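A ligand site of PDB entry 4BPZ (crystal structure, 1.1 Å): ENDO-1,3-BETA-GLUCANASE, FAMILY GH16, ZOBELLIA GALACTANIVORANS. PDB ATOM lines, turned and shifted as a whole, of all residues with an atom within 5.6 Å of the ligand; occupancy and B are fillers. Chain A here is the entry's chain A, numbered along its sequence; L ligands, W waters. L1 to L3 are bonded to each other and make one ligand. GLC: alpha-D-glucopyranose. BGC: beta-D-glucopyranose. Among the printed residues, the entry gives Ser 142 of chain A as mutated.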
ATOM      1  N   HIS A  43      -0.046  21.789 -23.472  1.00  0.00           N
ATOM      2  CA  HIS A  43       0.688  23.049 -23.430  1.00  0.00           C
ATOM      3  C   HIS A  43       1.699  23.044 -22.318  1.00  0.00           C
ATOM      4  O   HIS A  43       1.827  22.092 -21.538  1.00  0.00           O
ATOM      5  CB  HIS A  43      -0.293  24.189 -23.330  1.00  0.00           C
ATOM      6  CG  HIS A  43      -1.302  24.173 -24.450  1.00  0.00           C
ATOM      7  ND1 HIS A  43      -0.928  24.352 -25.754  1.00  0.00           N
ATOM      8  CD2 HIS A  43      -2.657  23.983 -24.409  1.00  0.00           C
ATOM      9  CE1 HIS A  43      -2.065  24.328 -26.521  1.00  0.00           C
ATOM     10  NE2 HIS A  43      -3.122  24.133 -25.670  1.00  0.00           N
ATOM     11  N   ASN A  44       2.427  24.174 -22.180  1.00  0.00           N
ATOM     12  CA  ASN A  44       3.306  24.384 -21.060  1.00  0.00           C
ATOM     13  C   ASN A  44       4.408  23.354 -20.932  1.00  0.00           C
ATOM     14  O   ASN A  44       4.901  23.105 -19.799  1.00  0.00           O
ATOM     15  CB  ASN A  44       2.516  24.513 -19.729  1.00  0.00           C
ATOM     16  CG  ASN A  44       1.363  25.451 -19.837  1.00  0.00           C
ATOM     17  OD1 ASN A  44       1.571  26.615 -20.224  1.00  0.00           O
ATOM     18  ND2 ASN A  44       0.165  25.008 -19.508  1.00  0.00           N
ATOM     19  N   GLU A  46       4.068  20.259 -20.732  1.00  0.00           N
ATOM     20  CA  GLU A  46       3.603  19.215 -19.813  1.00  0.00           C
ATOM     21  C   GLU A  46       3.892  17.858 -20.401  1.00  0.00           C
ATOM     22  O   GLU A  46       3.916  17.637 -21.623  1.00  0.00           O
ATOM     23  CB  GLU A  46       2.093  19.390 -19.639  1.00  0.00           C
ATOM     24  CG  GLU A  46       1.780  20.632 -18.818  1.00  0.00           C
ATOM     25  CD  GLU A  46       0.334  21.074 -18.985  1.00  0.00           C
ATOM     26  OE1 GLU A  46      -0.527  20.232 -19.407  1.00  0.00           O
ATOM     27  OE2 GLU A  46       0.062  22.263 -18.664  1.00  0.00           O
ATOM     28  N   ARG A  86      -8.303  15.378 -17.185  1.00  0.00           N
ATOM     29  CA  ARG A  86      -8.620  16.809 -17.350  1.00  0.00           C
ATOM     30  C   ARG A  86     -10.159  16.878 -17.609  1.00  0.00           C
ATOM     31  O   ARG A  86     -10.591  16.525 -18.709  1.00  0.00           O
ATOM     32  CB  ARG A  86      -7.815  17.443 -18.496  1.00  0.00           C
ATOM     33  CG  ARG A  86      -8.131  18.883 -18.773  1.00  0.00           C
ATOM     34  CD  ARG A  86      -7.041  19.454 -19.660  1.00  0.00           C
ATOM     35  NE  ARG A  86      -7.394  20.806 -20.171  1.00  0.00           N
ATOM     36  CZ  ARG A  86      -6.507  21.790 -20.334  1.00  0.00           C
ATOM     37  NH1 ARG A  86      -5.306  21.755 -19.804  1.00  0.00           N
ATOM     38  NH2 ARG A  86      -6.912  22.888 -20.999  1.00  0.00           N
ATOM     39  N   TRP A 111       1.144  19.126 -10.758  1.00  0.00           N
ATOM     40  CA  TRP A 111       0.633  20.474 -11.015  1.00  0.00           C
ATOM     41  C   TRP A 111      -0.873  20.416 -11.043  1.00  0.00           C
ATOM     42  O   TRP A 111      -1.483  20.372 -12.163  1.00  0.00           O
ATOM     43  CB  TRP A 111       1.270  21.013 -12.297  1.00  0.00           C
ATOM     44  CG  TRP A 111       0.848  22.376 -12.737  1.00  0.00           C
ATOM     45  CD1 TRP A 111       0.060  23.286 -12.078  1.00  0.00           C
ATOM     46  CD2 TRP A 111       1.204  22.957 -14.003  1.00  0.00           C
ATOM     47  NE1 TRP A 111      -0.104  24.432 -12.880  1.00  0.00           N
ATOM     48  CE2 TRP A 111       0.581  24.212 -14.048  1.00  0.00           C
ATOM     49  CE3 TRP A 111       2.007  22.547 -15.057  1.00  0.00           C
ATOM     50  CZ2 TRP A 111       0.748  25.068 -15.132  1.00  0.00           C
ATOM     51  CZ3 TRP A 111       2.190  23.411 -16.155  1.00  0.00           C
ATOM     52  CH2 TRP A 111       1.573  24.662 -16.164  1.00  0.00           C
ATOM     53  N   PRO A 112      -1.541  20.391  -9.935  1.00  0.00           N
ATOM     54  CA  PRO A 112      -3.017  20.374  -9.924  1.00  0.00           C
ATOM     55  C   PRO A 112      -3.546  21.770 -10.206  1.00  0.00           C
ATOM     56  O   PRO A 112      -2.894  22.782  -9.914  1.00  0.00           O
ATOM     57  CB  PRO A 112      -3.344  20.008  -8.450  1.00  0.00           C
ATOM     58  CG  PRO A 112      -2.199  20.676  -7.670  1.00  0.00           C
ATOM     59  CD  PRO A 112      -0.959  20.430  -8.532  1.00  0.00           C
ATOM     60  N   ALA A 113      -4.786  21.822 -10.720  1.00  0.00           N
ATOM     61  CA  ALA A 113      -5.416  23.093 -10.955  1.00  0.00           C
ATOM     62  C   ALA A 113      -6.936  22.970 -10.903  1.00  0.00           C
ATOM     63  O   ALA A 113      -7.525  21.952 -11.301  1.00  0.00           O
ATOM     64  CB  ALA A 113      -5.017  23.670 -12.293  1.00  0.00           C
ATOM     65  N   TRP A 115      -9.695  25.751 -12.350  1.00  0.00           N
ATOM     66  CA  TRP A 115      -9.566  27.002 -13.107  1.00  0.00           C
ATOM     67  C   TRP A 115     -10.698  27.078 -14.108  1.00  0.00           C
ATOM     68  O   TRP A 115     -11.532  26.182 -14.187  1.00  0.00           O
ATOM     69  CB  TRP A 115      -8.179  27.077 -13.759  1.00  0.00           C
ATOM     70  CG  TRP A 115      -7.828  25.948 -14.699  1.00  0.00           C
ATOM     71  CD1 TRP A 115      -7.643  24.632 -14.428  1.00  0.00           C
ATOM     72  CD2 TRP A 115      -7.469  26.096 -16.083  1.00  0.00           C
ATOM     73  NE1 TRP A 115      -7.201  23.946 -15.512  1.00  0.00           N
ATOM     74  CE2 TRP A 115      -7.085  24.830 -16.537  1.00  0.00           C
ATOM     75  CE3 TRP A 115      -7.406  27.188 -16.980  1.00  0.00           C
ATOM     76  CZ2 TRP A 115      -6.572  24.597 -17.842  1.00  0.00           C
ATOM     77  CZ3 TRP A 115      -6.930  26.981 -18.255  1.00  0.00           C
ATOM     78  CH2 TRP A 115      -6.505  25.706 -18.709  1.00  0.00           C
ATOM     79  N   LEU A 117     -12.020  28.609 -18.157  1.00  0.00           N
ATOM     80  CA  LEU A 117     -11.781  29.189 -19.466  1.00  0.00           C
ATOM     81  C   LEU A 117     -13.089  29.839 -19.922  1.00  0.00           C
ATOM     82  O   LEU A 117     -14.184  29.278 -19.701  1.00  0.00           O
ATOM     83  CB  LEU A 117     -11.358  28.155 -20.505  1.00  0.00           C
ATOM     84  CG  LEU A 117      -9.904  27.690 -20.482  1.00  0.00           C
ATOM     85  CD1 LEU A 117      -9.661  26.462 -21.288  1.00  0.00           C
ATOM     86  CD2 LEU A 117      -9.020  28.867 -20.885  1.00  0.00           C
ATOM     87  N   GLU A 123     -11.303  25.548 -27.372  1.00  0.00           N
ATOM     88  CA  GLU A 123     -10.179  24.673 -27.189  1.00  0.00           C
ATOM     89  C   GLU A 123     -10.452  23.330 -27.780  1.00  0.00           C
ATOM     90  O   GLU A 123     -11.574  22.753 -27.667  1.00  0.00           O
ATOM     91  CB  GLU A 123      -9.855  24.526 -25.674  1.00  0.00           C
ATOM     92  CG  GLU A 123      -8.796  23.487 -25.433  1.00  0.00           C
ATOM     93  CD  GLU A 123      -8.192  23.659 -24.083  1.00  0.00           C
ATOM     94  OE1 GLU A 123      -7.295  24.544 -23.927  1.00  0.00           O
ATOM     95  OE2 GLU A 123      -8.661  23.012 -23.099  1.00  0.00           O
ATOM     96  N   GLU A 136      -9.387  32.495 -29.260  1.00  0.00           N
ATOM     97  CA  GLU A 136      -8.294  31.661 -28.834  1.00  0.00           C
ATOM     98  C   GLU A 136      -7.663  32.245 -27.574  1.00  0.00           C
ATOM     99  O   GLU A 136      -7.411  33.455 -27.475  1.00  0.00           O
ATOM    100  CB  GLU A 136      -7.254  31.668 -29.997  1.00  0.00           C
ATOM    101  CG  GLU A 136      -6.025  30.866 -29.610  1.00  0.00           C
ATOM    102  CD  GLU A 136      -5.176  30.540 -30.813  1.00  0.00           C
ATOM    103  OE1 GLU A 136      -5.472  29.585 -31.581  1.00  0.00           O
ATOM    104  OE2 GLU A 136      -4.195  31.268 -31.015  1.00  0.00           O
ATOM    105  N   TRP A 137      -7.364  31.373 -26.595  1.00  0.00           N
ATOM    106  CA  TRP A 137      -6.688  31.806 -25.382  1.00  0.00           C
ATOM    107  C   TRP A 137      -5.463  32.656 -25.743  1.00  0.00           C
ATOM    108  O   TRP A 137      -4.754  32.246 -26.649  1.00  0.00           O
ATOM    109  CB  TRP A 137      -6.204  30.537 -24.601  1.00  0.00           C
ATOM    110  CG  TRP A 137      -5.599  30.876 -23.289  1.00  0.00           C
ATOM    111  CD1 TRP A 137      -6.176  30.863 -22.066  1.00  0.00           C
ATOM    112  CD2 TRP A 137      -4.204  31.233 -23.076  1.00  0.00           C
ATOM    113  NE1 TRP A 137      -5.304  31.209 -21.099  1.00  0.00           N
ATOM    114  CE2 TRP A 137      -4.077  31.438 -21.678  1.00  0.00           C
ATOM    115  CE3 TRP A 137      -3.087  31.373 -23.917  1.00  0.00           C
ATOM    116  CZ2 TRP A 137      -2.832  31.822 -21.110  1.00  0.00           C
ATOM    117  CZ3 TRP A 137      -1.878  31.756 -23.357  1.00  0.00           C
ATOM    118  CH2 TRP A 137      -1.756  31.974 -21.978  1.00  0.00           C
ATOM    119  N   SER A 142      -9.214  33.522 -18.646  1.00  0.00           N
ATOM    120  CA  SER A 142      -9.153  32.431 -17.727  1.00  0.00           C
ATOM    121  C   SER A 142      -8.899  32.915 -16.328  1.00  0.00           C
ATOM    122  O   SER A 142      -8.237  33.941 -16.113  1.00  0.00           O
ATOM    123  CB  SER A 142      -7.942  31.779 -18.166  1.00  0.00           C
ATOM    124  OG  SER A 142      -7.683  30.641 -17.355  1.00  0.00           O
ATOM    125  N   ILE A 143      -9.504  32.208 -15.370  1.00  0.00           N
ATOM    126  CA  ILE A 143      -9.316  32.429 -13.970  1.00  0.00           C
ATOM    127  C   ILE A 143      -8.731  31.198 -13.307  1.00  0.00           C
ATOM    128  O   ILE A 143      -9.308  30.093 -13.414  1.00  0.00           O
ATOM    129  CB  ILE A 143     -10.615  32.713 -13.297  1.00  0.00           C
ATOM    130  CG1 ILE A 143     -11.343  33.886 -13.980  1.00  0.00           C
ATOM    131  CG2 ILE A 143     -10.472  33.017 -11.770  1.00  0.00           C
ATOM    132  CD1 ILE A 143     -12.748  34.129 -13.531  1.00  0.00           C
ATOM    133  N   ASP A 144      -7.601  31.353 -12.622  1.00  0.00           N
ATOM    134  CA  ASP A 144      -7.092  30.229 -11.795  1.00  0.00           C
ATOM    135  C   ASP A 144      -7.770  30.437 -10.479  1.00  0.00           C
ATOM    136  O   ASP A 144      -7.761  31.576  -9.933  1.00  0.00           O
ATOM    137  CB  ASP A 144      -5.494  30.180 -11.846  1.00  0.00           C
ATOM    138  CG  ASP A 144      -5.071  29.876 -13.312  1.00  0.00           C
ATOM    139  OD1 ASP A 144      -5.091  28.484 -13.594  1.00  0.00           O
ATOM    140  OD2 ASP A 144      -4.288  30.515 -13.905  1.00  0.00           O
ATOM    141  N   GLU A 147      -3.836  26.820  -8.286  1.00  0.00           N
ATOM    142  CA  GLU A 147      -2.797  25.987  -8.809  1.00  0.00           C
ATOM    143  C   GLU A 147      -1.774  25.744  -7.708  1.00  0.00           C
ATOM    144  O   GLU A 147      -1.607  26.573  -6.809  1.00  0.00           O
ATOM    145  CB  GLU A 147      -2.072  26.621  -9.977  1.00  0.00           C
ATOM    146  CG  GLU A 147      -2.939  26.980 -11.168  1.00  0.00           C
ATOM    147  CD  GLU A 147      -2.119  27.649 -12.277  1.00  0.00           C
ATOM    148  OE1 GLU A 147      -1.383  26.995 -13.037  1.00  0.00           O
ATOM    149  OE2 GLU A 147      -2.123  28.952 -12.357  1.00  0.00           O
ATOM    150  N   HIS A 159      -4.371  33.120 -10.180  1.00  0.00           N
ATOM    151  CA  HIS A 159      -3.843  33.907 -11.296  1.00  0.00           C
ATOM    152  C   HIS A 159      -4.708  34.053 -12.538  1.00  0.00           C
ATOM    153  O   HIS A 159      -5.233  33.099 -13.023  1.00  0.00           O
ATOM    154  CB  HIS A 159      -2.781  33.115 -11.873  1.00  0.00           C
ATOM    155  CG  HIS A 159      -1.605  33.872 -12.086  1.00  0.00           C
ATOM    156  ND1 HIS A 159      -1.213  34.447 -13.246  1.00  0.00           N
ATOM    157  CD2 HIS A 159      -0.630  34.167 -11.165  1.00  0.00           C
ATOM    158  CE1 HIS A 159       0.001  35.060 -13.023  1.00  0.00           C
ATOM    159  NE2 HIS A 159       0.353  34.856 -11.795  1.00  0.00           N
ATOM    160  N   HIS A 161      -5.419  35.236 -16.517  1.00  0.00           N
ATOM    161  CA  HIS A 161      -4.757  35.311 -17.848  1.00  0.00           C
ATOM    162  C   HIS A 161      -5.774  35.801 -18.838  1.00  0.00           C
ATOM    163  O   HIS A 161      -6.855  35.161 -18.970  1.00  0.00           O
ATOM    164  CB  HIS A 161      -4.226  33.960 -18.300  1.00  0.00           C
ATOM    165  CG  HIS A 161      -3.274  33.284 -17.373  1.00  0.00           C
ATOM    166  ND1 HIS A 161      -3.599  32.591 -16.214  1.00  0.00           N
ATOM    167  CD2 HIS A 161      -1.911  33.347 -17.389  1.00  0.00           C
ATOM    168  CE1 HIS A 161      -2.463  32.166 -15.636  1.00  0.00           C
ATOM    169  NE2 HIS A 161      -1.474  32.602 -16.335  1.00  0.00           N
ATOM    170  N   TYR A 170      -1.409  40.739 -23.904  1.00  0.00           N
ATOM    171  CA  TYR A 170      -1.585  39.657 -22.936  1.00  0.00           C
ATOM    172  C   TYR A 170      -1.353  40.104 -21.526  1.00  0.00           C
ATOM    173  O   TYR A 170      -0.296  40.696 -21.241  1.00  0.00           O
ATOM    174  CB  TYR A 170      -0.668  38.500 -23.294  1.00  0.00           C
ATOM    175  CG  TYR A 170      -0.548  37.380 -22.313  1.00  0.00           C
ATOM    176  CD1 TYR A 170      -1.661  36.697 -21.909  1.00  0.00           C
ATOM    177  CD2 TYR A 170       0.687  36.948 -21.792  1.00  0.00           C
ATOM    178  CE1 TYR A 170      -1.599  35.676 -20.971  1.00  0.00           C
ATOM    179  CE2 TYR A 170       0.771  35.865 -20.907  1.00  0.00           C
ATOM    180  CZ  TYR A 170      -0.373  35.208 -20.495  1.00  0.00           C
ATOM    181  OH  TYR A 170      -0.220  34.172 -19.621  1.00  0.00           O
ATOM    182  N   ASN A 227      -7.825  19.329 -13.108  1.00  0.00           N
ATOM    183  CA  ASN A 227      -6.821  18.472 -13.747  1.00  0.00           C
ATOM    184  C   ASN A 227      -5.605  18.292 -12.832  1.00  0.00           C
ATOM    185  O   ASN A 227      -5.405  19.102 -11.912  1.00  0.00           O
ATOM    186  CB  ASN A 227      -6.367  19.007 -15.109  1.00  0.00           C
ATOM    187  CG  ASN A 227      -5.625  20.302 -15.008  1.00  0.00           C
ATOM    188  OD1 ASN A 227      -6.258  21.343 -14.778  1.00  0.00           O
ATOM    189  ND2 ASN A 227      -4.312  20.275 -15.045  1.00  0.00           N
HETATM  190  C1  GLC L   1      -3.286  28.634 -16.082  1.00  0.00           C
HETATM  191  C2  GLC L   1      -2.387  28.569 -17.372  1.00  0.00           C
HETATM  192  C3  GLC L   1      -2.827  27.330 -18.154  1.00  0.00           C
HETATM  193  C4  GLC L   1      -2.748  26.128 -17.315  1.00  0.00           C
HETATM  194  C5  GLC L   1      -3.783  26.342 -16.234  1.00  0.00           C
HETATM  195  C6  GLC L   1      -3.885  25.200 -15.242  1.00  0.00           C
HETATM  196  O1  GLC L   1      -4.585  29.122 -16.337  1.00  0.00           O
HETATM  197  O2  GLC L   1      -2.588  29.768 -18.064  1.00  0.00           O
HETATM  198  O3  GLC L   1      -1.953  27.182 -19.344  1.00  0.00           O
HETATM  199  O4  GLC L   1      -3.038  24.947 -18.099  1.00  0.00           O
HETATM  200  O5  GLC L   1      -3.383  27.499 -15.465  1.00  0.00           O
HETATM  201  O6  GLC L   1      -2.655  24.963 -14.572  1.00  0.00           O
HETATM  202  C2  BGC L   2      -1.227  27.679 -21.558  1.00  0.00           C
HETATM  203  C3  BGC L   2      -1.679  28.211 -22.889  1.00  0.00           C
HETATM  204  C4  BGC L   2      -3.024  27.510 -23.326  1.00  0.00           C
HETATM  205  C5  BGC L   2      -4.081  27.654 -22.201  1.00  0.00           C
HETATM  206  C6  BGC L   2      -5.355  26.871 -22.444  1.00  0.00           C
HETATM  207  C1  BGC L   2      -2.393  27.794 -20.549  1.00  0.00           C
HETATM  208  O2  BGC L   2      -0.114  28.413 -21.142  1.00  0.00           O
HETATM  209  O3  BGC L   2      -0.672  27.870 -23.838  1.00  0.00           O
HETATM  210  O4  BGC L   2      -3.641  28.136 -24.453  1.00  0.00           O
HETATM  211  O5  BGC L   2      -3.512  27.064 -21.001  1.00  0.00           O
HETATM  212  O6  BGC L   2      -5.170  25.477 -22.511  1.00  0.00           O
HETATM  213  C2  BGC L   3      -4.272  28.023 -26.762  1.00  0.00           C
HETATM  214  C3  BGC L   3      -3.784  27.582 -28.104  1.00  0.00           C
HETATM  215  C4  BGC L   3      -2.464  28.278 -28.477  1.00  0.00           C
HETATM  216  C5  BGC L   3      -1.472  28.088 -27.301  1.00  0.00           C
HETATM  217  C6  BGC L   3      -0.147  28.738 -27.620  1.00  0.00           C
HETATM  218  C1  BGC L   3      -3.203  27.764 -25.726  1.00  0.00           C
HETATM  219  O2  BGC L   3      -5.468  27.333 -26.438  1.00  0.00           O
HETATM  220  O3  BGC L   3      -4.694  27.936 -29.097  1.00  0.00           O
HETATM  221  O4  BGC L   3      -1.944  27.683 -29.638  1.00  0.00           O
HETATM  222  O5  BGC L   3      -2.053  28.537 -26.065  1.00  0.00           O
HETATM  223  O6  BGC L   3       0.752  28.402 -26.555  1.00  0.00           O
HETATM  224  O   HOH W   1      -2.052  22.680 -17.036  1.00  0.00           O
HETATM  225  O   HOH W   2      -3.806  26.976 -31.560  1.00  0.00           O
HETATM  226  O   HOH W   3      -3.720  24.098 -20.592  1.00  0.00           O
HETATM  227  O   HOH W   4      -7.441  27.414 -24.877  1.00  0.00           O
HETATM  228  O   HOH W   5      -8.491  28.671 -26.924  1.00  0.00           O
HETATM  229  O   HOH W   6      -5.619  24.634 -26.321  1.00  0.00           O
HETATM  230  O   HOH W   7      -5.151  30.607 -18.506  1.00  0.00           O
HETATM  231  O   HOH W   8      -7.289  27.060 -28.916  1.00  0.00           O
HETATM  232  O   HOH W   9      -2.395  24.595 -29.729  1.00  0.00           O
HETATM  233  O   HOH W  10       1.070  28.736 -16.878  1.00  0.00           O
HETATM  234  O   HOH W  11       1.539  30.224 -22.699  1.00  0.00           O
HETATM  235  O   HOH W  12      -6.202  31.938 -15.427  1.00  0.00           O
HETATM  236  O   HOH W  13      -0.091  30.311 -18.994  1.00  0.00           O
HETATM  237  O   HOH W  14       1.990  26.650 -23.693  1.00  0.00           O
HETATM  238  O   HOH W  15      -2.275  22.266 -14.303  1.00  0.00           O
HETATM  239  O   HOH W  16       1.632  25.103 -26.625  1.00  0.00           O
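An oxygen (O2) of BGC L2 lies within hydrogen-bond range of the side-chain amide oxygen (OD1) of Asn 44, 2.6 Å away. The side-chain carboxylate (OD2) of Asp 144 is in hydrogen-bond range of an oxygen (O1) of GLC L1 (2.8 Å). OE1 of Glu 123 is in hydrogen-bond range of O6 of BGC L2 (2.7 Å). The side-chain carboxylate of Glu 147 sits at hydrogen-bond distance from an oxygen (O6) of GLC L1 (2.8 Å). OE1 of Glu 136 lies within hydrogen-bond range of O3 of BGC L3, 3.1 Å away. The indole nitrogen (NE1) of Trp 111 is in hydrogen-bond range of an oxygen (O6) of GLC L1 (3.1 Å). The guanidinium group (NH2) of Arg 86 is in hydrogen-bond range of an oxygen (O6) of BGC L2, at 3.5 Å.
ND2 of Asn 44 is in hydrogen-bond range of OE2 of Glu 46, at 2.9 Å. A ring nitrogen (ND1) of His 161 lies close to the side-chain carboxylate (OD2) of Asp 144 (3.2 Å). N of Asp 144 lies within hydrogen-bond range of O of His 159 (3.0 Å). The side-chain carboxylate of Glu 123 lies within salt-bridge range of the guanidinium group of Arg 86, at 2.7 Å. NE1 of Trp 111 sits at hydrogen-bond distance from OE1 of Glu 147 (2.9 Å). N of Ser 142 lies within hydrogen-bond range of O of His 161 (2.9 Å). NE1 of Trp 115 lies within hydrogen-bond range of OD1 of Asn 227 (2.9 Å). N of Ala 113 is in hydrogen-bond range of O of Asn 227 (3.0 Å).
CD2 of His 43 touches O6 of BGC L2 (3.5 Å). Ala 113 touches the ligand. CE2 of Trp 115 touches C6 of GLC L1, 3.5 Å away. CE3 of Trp 137 touches O4 of BGC L2, at 3.3 Å. OG of Ser 142 touches O1 of GLC L1 (3.6 Å). CE1 of His 161 touches O2 of GLC L1, at 3.4 Å. Hydrophobic or aromatic side chains that line the ligand: His 43, Trp 111, Ala 113, Trp 115, Trp 137 and His 161. The nearest printed residue that does not touch the ligand is Glu 46 (4.1 Å).
Water W7 lies within hydrogen-bond range of the indole nitrogen (NE1) of Trp 137 (2.7 Å), an oxygen (O1) of GLC L1 (2.7 Å), the side-chain hydroxyl (OG) of Ser 142 (2.8 Å) and a ring nitrogen (ND1) of His 161 (3.4 Å). Water W15 lies within hydrogen-bond range of O6 of GLC L1, ND2 of Asn 227 and O of Trp 111. Water W2 bridges an oxygen (O4) of BGC L3 and the side-chain carboxylate (OE1) of Glu 136. Water W5 lies within hydrogen-bond range of N of Trp 137 (2.9 Å) and O2 of BGC L3 (3.3 Å). Water W12 lies within hydrogen-bond range of OG of Ser 142 (2.8 Å), ND1 of His 161 (2.8 Å), OD2 of Asp 144 (2.8 Å), O of His 159 (2.8 Å), N of Ile 143 (3.3 Å) and O1 of GLC L1 (3.4 Å). Water W16 bridges a ring nitrogen (ND1) of His 43 (2.8 Å) and an oxygen (O6) of BGC L3 (3.4 Å).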
